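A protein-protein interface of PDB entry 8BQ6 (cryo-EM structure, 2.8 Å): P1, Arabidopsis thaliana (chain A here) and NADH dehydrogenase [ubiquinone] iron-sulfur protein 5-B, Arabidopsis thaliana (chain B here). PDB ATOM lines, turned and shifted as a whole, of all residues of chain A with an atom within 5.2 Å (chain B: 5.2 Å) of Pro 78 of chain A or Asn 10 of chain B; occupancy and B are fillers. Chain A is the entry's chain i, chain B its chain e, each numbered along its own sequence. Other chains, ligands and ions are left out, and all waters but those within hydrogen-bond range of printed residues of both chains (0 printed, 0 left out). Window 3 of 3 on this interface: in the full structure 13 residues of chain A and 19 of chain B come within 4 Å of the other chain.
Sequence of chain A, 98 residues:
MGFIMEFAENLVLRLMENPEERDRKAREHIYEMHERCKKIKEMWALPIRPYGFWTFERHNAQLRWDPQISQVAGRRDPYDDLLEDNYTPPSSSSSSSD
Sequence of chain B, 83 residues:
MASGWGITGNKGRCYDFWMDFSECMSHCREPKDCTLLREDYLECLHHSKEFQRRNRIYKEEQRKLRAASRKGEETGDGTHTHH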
ATOM      1  N   GLY A  74      23.145  25.473   1.778  1.00  0.00           N
ATOM      2  CA  GLY A  74      23.415  26.687   2.508  1.00  0.00           C
ATOM      3  C   GLY A  74      22.756  27.916   1.923  1.00  0.00           C
ATOM      4  O   GLY A  74      22.663  28.937   2.614  1.00  0.00           O
ATOM      5  N   ARG A  75      22.304  27.856   0.663  1.00  0.00           N
ATOM      6  CA  ARG A  75      21.630  29.005   0.066  1.00  0.00           C
ATOM      7  C   ARG A  75      20.449  28.608  -0.815  1.00  0.00           C
ATOM      8  O   ARG A  75      20.049  29.392  -1.684  1.00  0.00           O
ATOM      9  CB  ARG A  75      22.614  29.863  -0.740  1.00  0.00           C
ATOM     10  CG  ARG A  75      23.335  29.162  -1.874  1.00  0.00           C
ATOM     11  CD  ARG A  75      24.400  30.075  -2.464  1.00  0.00           C
ATOM     12  NE  ARG A  75      23.835  31.252  -3.113  1.00  0.00           N
ATOM     13  CZ  ARG A  75      24.189  32.502  -2.844  1.00  0.00           C
ATOM     14  NH1 ARG A  75      25.070  32.784  -1.900  1.00  0.00           N
ATOM     15  NH2 ARG A  75      23.638  33.494  -3.536  1.00  0.00           N
ATOM     16  N   ARG A  76      19.872  27.432  -0.612  1.00  0.00           N
ATOM     17  CA  ARG A  76      18.749  26.989  -1.420  1.00  0.00           C
ATOM     18  C   ARG A  76      17.426  27.424  -0.813  1.00  0.00           C
ATOM     19  O   ARG A  76      17.292  27.568   0.405  1.00  0.00           O
ATOM     20  CB  ARG A  76      18.756  25.473  -1.566  1.00  0.00           C
ATOM     21  CG  ARG A  76      20.098  24.948  -1.958  1.00  0.00           C
ATOM     22  CD  ARG A  76      20.028  23.513  -2.356  1.00  0.00           C
ATOM     23  NE  ARG A  76      19.229  23.318  -3.556  1.00  0.00           N
ATOM     24  CZ  ARG A  76      18.831  22.131  -3.988  1.00  0.00           C
ATOM     25  NH1 ARG A  76      19.177  21.020  -3.360  1.00  0.00           N
ATOM     26  NH2 ARG A  76      18.078  22.055  -5.080  1.00  0.00           N
ATOM     27  N   ASP A  77      16.449  27.631  -1.683  1.00  0.00           N
ATOM     28  CA  ASP A  77      15.069  27.706  -1.241  1.00  0.00           C
ATOM     29  C   ASP A  77      14.717  26.397  -0.542  1.00  0.00           C
ATOM     30  O   ASP A  77      15.061  25.320  -1.047  1.00  0.00           O
ATOM     31  CB  ASP A  77      14.156  27.960  -2.442  1.00  0.00           C
ATOM     32  CG  ASP A  77      12.696  28.149  -2.061  1.00  0.00           C
ATOM     33  OD1 ASP A  77      12.352  28.109  -0.863  1.00  0.00           O
ATOM     34  OD2 ASP A  77      11.880  28.350  -2.983  1.00  0.00           O
ATOM     35  N   PRO A  78      14.082  26.442   0.632  1.00  0.00           N
ATOM     36  CA  PRO A  78      13.808  25.193   1.363  1.00  0.00           C
ATOM     37  C   PRO A  78      12.948  24.195   0.606  1.00  0.00           C
ATOM     38  O   PRO A  78      13.088  22.988   0.831  1.00  0.00           O
ATOM     39  CB  PRO A  78      13.117  25.685   2.644  1.00  0.00           C
ATOM     40  CG  PRO A  78      12.706  27.100   2.359  1.00  0.00           C
ATOM     41  CD  PRO A  78      13.739  27.629   1.429  1.00  0.00           C
ATOM     42  N   TYR A  79      12.064  24.648  -0.284  1.00  0.00           N
ATOM     43  CA  TYR A  79      11.211  23.709  -1.003  1.00  0.00           C
ATOM     44  C   TYR A  79      11.977  22.890  -2.033  1.00  0.00           C
ATOM     45  O   TYR A  79      11.470  21.855  -2.480  1.00  0.00           O
ATOM     46  CB  TYR A  79      10.054  24.458  -1.663  1.00  0.00           C
ATOM     47  CG  TYR A  79       9.008  24.858  -0.656  1.00  0.00           C
ATOM     48  CD1 TYR A  79       8.214  23.899  -0.049  1.00  0.00           C
ATOM     49  CD2 TYR A  79       8.847  26.181  -0.274  1.00  0.00           C
ATOM     50  CE1 TYR A  79       7.271  24.244   0.886  1.00  0.00           C
ATOM     51  CE2 TYR A  79       7.903  26.537   0.667  1.00  0.00           C
ATOM     52  CZ  TYR A  79       7.117  25.562   1.243  1.00  0.00           C
ATOM     53  OH  TYR A  79       6.171  25.896   2.181  1.00  0.00           O
ATOM     54  N   ASP A  80      13.187  23.313  -2.401  1.00  0.00           N
ATOM     55  CA  ASP A  80      13.955  22.593  -3.411  1.00  0.00           C
ATOM     56  C   ASP A  80      14.318  21.188  -2.959  1.00  0.00           C
ATOM     57  O   ASP A  80      14.424  20.278  -3.787  1.00  0.00           O
ATOM     58  CB  ASP A  80      15.222  23.367  -3.756  1.00  0.00           C
ATOM     59  CG  ASP A  80      14.935  24.621  -4.541  1.00  0.00           C
ATOM     60  OD1 ASP A  80      14.254  24.528  -5.579  1.00  0.00           O
ATOM     61  OD2 ASP A  80      15.404  25.698  -4.131  1.00  0.00           O
ATOM     62  N   ASP A  81      14.537  20.997  -1.660  1.00  0.00           N
ATOM     63  CA  ASP A  81      14.873  19.669  -1.166  1.00  0.00           C
ATOM     64  C   ASP A  81      13.659  18.751  -1.191  1.00  0.00           C
ATOM     65  O   ASP A  81      13.796  17.531  -1.340  1.00  0.00           O
ATOM     66  CB  ASP A  81      15.440  19.770   0.247  1.00  0.00           C
ATOM     67  CG  ASP A  81      16.950  19.776   0.265  1.00  0.00           C
ATOM     68  OD1 ASP A  81      17.529  19.776   1.371  1.00  0.00           O
ATOM     69  OD2 ASP A  81      17.557  19.783  -0.827  1.00  0.00           O
ATOM     70  N   LEU A  82      12.460  19.320  -1.044  1.00  0.00           N
ATOM     71  CA  LEU A  82      11.258  18.498  -0.982  1.00  0.00           C
ATOM     72  C   LEU A  82      10.867  17.955  -2.348  1.00  0.00           C
ATOM     73  O   LEU A  82      10.247  16.889  -2.435  1.00  0.00           O
ATOM     74  CB  LEU A  82      10.097  19.292  -0.383  1.00  0.00           C
ATOM     75  CG  LEU A  82      10.225  19.733   1.078  1.00  0.00           C
ATOM     76  CD1 LEU A  82       9.059  20.631   1.468  1.00  0.00           C
ATOM     77  CD2 LEU A  82      10.357  18.565   2.026  1.00  0.00           C
ATOM     78  N   GLY B   4      23.116  35.965  -0.069  1.00  0.00           N
ATOM     79  CA  GLY B   4      22.316  34.759  -0.350  1.00  0.00           C
ATOM     80  C   GLY B   4      22.411  33.713   0.737  1.00  0.00           C
ATOM     81  O   GLY B   4      21.511  32.871   0.812  1.00  0.00           O
ATOM     82  N   TRP B   5      23.460  33.768   1.553  1.00  0.00           N
ATOM     83  CA  TRP B   5      23.664  32.725   2.550  1.00  0.00           C
ATOM     84  C   TRP B   5      22.859  33.095   3.789  1.00  0.00           C
ATOM     85  O   TRP B   5      23.151  34.099   4.448  1.00  0.00           O
ATOM     86  CB  TRP B   5      25.143  32.578   2.898  1.00  0.00           C
ATOM     87  CG  TRP B   5      26.075  32.354   1.742  1.00  0.00           C
ATOM     88  CD1 TRP B   5      26.884  33.281   1.156  1.00  0.00           C
ATOM     89  CD2 TRP B   5      26.322  31.121   1.061  1.00  0.00           C
ATOM     90  NE1 TRP B   5      27.610  32.705   0.146  1.00  0.00           N
ATOM     91  CE2 TRP B   5      27.283  31.378   0.067  1.00  0.00           C
ATOM     92  CE3 TRP B   5      25.820  29.825   1.192  1.00  0.00           C
ATOM     93  CZ2 TRP B   5      27.751  30.391  -0.789  1.00  0.00           C
ATOM     94  CZ3 TRP B   5      26.284  28.849   0.341  1.00  0.00           C
ATOM     95  CH2 TRP B   5      27.241  29.134  -0.636  1.00  0.00           C
ATOM     96  N   GLY B   6      21.839  32.303   4.107  1.00  0.00           N
ATOM     97  CA  GLY B   6      21.056  32.565   5.294  1.00  0.00           C
ATOM     98  C   GLY B   6      21.673  31.965   6.542  1.00  0.00           C
ATOM     99  O   GLY B   6      22.420  30.989   6.494  1.00  0.00           O
ATOM    100  N   ILE B   7      21.338  32.559   7.691  1.00  0.00           N
ATOM    101  CA  ILE B   7      21.964  32.156   8.947  1.00  0.00           C
ATOM    102  C   ILE B   7      21.475  30.814   9.465  1.00  0.00           C
ATOM    103  O   ILE B   7      22.047  30.297  10.430  1.00  0.00           O
ATOM    104  CB  ILE B   7      21.768  33.231  10.035  1.00  0.00           C
ATOM    105  CG1 ILE B   7      20.302  33.311  10.457  1.00  0.00           C
ATOM    106  CG2 ILE B   7      22.312  34.576   9.571  1.00  0.00           C
ATOM    107  CD1 ILE B   7      20.051  34.261  11.592  1.00  0.00           C
ATOM    108  N   THR B   8      20.440  30.234   8.859  1.00  0.00           N
ATOM    109  CA  THR B   8      19.981  28.896   9.213  1.00  0.00           C
ATOM    110  C   THR B   8      20.257  27.880   8.113  1.00  0.00           C
ATOM    111  O   THR B   8      19.747  26.757   8.181  1.00  0.00           O
ATOM    112  CB  THR B   8      18.484  28.898   9.541  1.00  0.00           C
ATOM    113  OG1 THR B   8      17.770  29.594   8.514  1.00  0.00           O
ATOM    114  CG2 THR B   8      18.235  29.584  10.868  1.00  0.00           C
ATOM    115  N   GLY B   9      21.041  28.240   7.103  1.00  0.00           N
ATOM    116  CA  GLY B   9      21.403  27.296   6.068  1.00  0.00           C
ATOM    117  C   GLY B   9      20.477  27.245   4.880  1.00  0.00           C
ATOM    118  O   GLY B   9      20.439  26.222   4.187  1.00  0.00           O
ATOM    119  N   ASN B  10      19.718  28.304   4.625  1.00  0.00           N
ATOM    120  CA  ASN B  10      18.864  28.402   3.455  1.00  0.00           C
ATOM    121  C   ASN B  10      19.048  29.774   2.835  1.00  0.00           C
ATOM    122  O   ASN B  10      19.771  30.622   3.360  1.00  0.00           O
ATOM    123  CB  ASN B  10      17.395  28.168   3.811  1.00  0.00           C
ATOM    124  CG  ASN B  10      17.081  26.716   4.010  1.00  0.00           C
ATOM    125  OD1 ASN B  10      17.118  25.926   3.070  1.00  0.00           O
ATOM    126  ND2 ASN B  10      16.785  26.344   5.245  1.00  0.00           N
ATOM    127  N   LYS B  11      18.380  29.987   1.709  1.00  0.00           N
ATOM    128  CA  LYS B  11      18.437  31.274   1.039  1.00  0.00           C
ATOM    129  C   LYS B  11      17.976  32.377   1.983  1.00  0.00           C
ATOM    130  O   LYS B  11      16.970  32.232   2.682  1.00  0.00           O
ATOM    131  CB  LYS B  11      17.570  31.245  -0.215  1.00  0.00           C
ATOM    132  CG  LYS B  11      17.568  32.542  -0.981  1.00  0.00           C
ATOM    133  CD  LYS B  11      16.520  32.531  -2.074  1.00  0.00           C
ATOM    134  CE  LYS B  11      16.945  31.655  -3.233  1.00  0.00           C
ATOM    135  NZ  LYS B  11      16.111  31.911  -4.435  1.00  0.00           N
ATOM    136  N   GLY B  12      18.730  33.472   2.010  1.00  0.00           N
ATOM    137  CA  GLY B  12      18.428  34.584   2.886  1.00  0.00           C
ATOM    138  C   GLY B  12      17.059  35.180   2.640  1.00  0.00           C
ATOM    139  O   GLY B  12      16.557  35.162   1.513  1.00  0.00           O
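O of Gly 74 of chain A lies close to O of Asn 10 of chain B (3.4 Å). The backbone NH (N) of Lys 11 of chain B sits at hydrogen-bond distance from the backbone carbonyl oxygen (O) of Arg 76 of chain A. The backbone carbonyl oxygen of Arg 76 of chain A sits close to the side-chain amide oxygen of Asn 10 of chain B, at 3.1 Å. The guanidinium group of Arg 75 of chain A lies close to the indole nitrogen of Trp 5 of chain B (3.3 Å).
The side-chain carboxylate (OD2) of Asp 81 of chain A is in salt-bridge range of the guanidinium group (NH1) of Arg 76 of chain A (3.3 Å). O of Gly 4 of chain B sits at hydrogen-bond distance from N of Gly 12 of chain B.
Among the printed residues, merely in contact across the chains: Arg 75 of chain A with Lys 11 of chain B (3.4 Å), Gly 74 of chain A with Gly 9 of chain B (3.4 Å), Arg 75 of chain A with Gly 4 of chain B (3.6 Å), Gly 74 of chain A with Trp 5 of chain B (3.6 Å), Gly 74 of chain A with Gly 6 of chain B (3.8 Å), Pro 78 of chain A with Asn 10 of chain B (3.8 Å) and Arg 75 of chain A with Asn 10 of chain B (3.9 Å).
Printed residues of chain B within 4 Å of Arg 75 of chain A: Gly 4, Trp 5, Asn 10 and Lys 11. Asp 77 of chain A touches none of the printed residues of chain B. Of the printed residues of chain A, Gly 4 of chain B touches Arg 75. Of the printed residues of chain A, Trp 5 of chain B touches Gly 74 (3.6 Å) and Arg 75 (3.3 Å). Printed residues of chain A within 4 Å of Gly 9 of chain B: Gly 74. Asn 10 of chain B touches just these residues of chain A: Gly 74 (3.4 Å), Arg 75 (3.9 Å), Arg 76 (3.1 Å) and Pro 78 (3.8 Å). Printed residues of chain A within 4 Å of Lys 11 of chain B: Arg 75 and Arg 76. The nearest residue of chain A that does not touch Asn 10 of chain B is Asp 77 of chain A (4.4 Å).
Of the 9 printed residues of chain A, 4 touch a printed residue of chain B. Of the 9 printed residues of chain B, 6 touch a printed residue of chain A. Hydrophobic or aromatic side chains of chain B that line the printed part of chain A: Trp 5.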
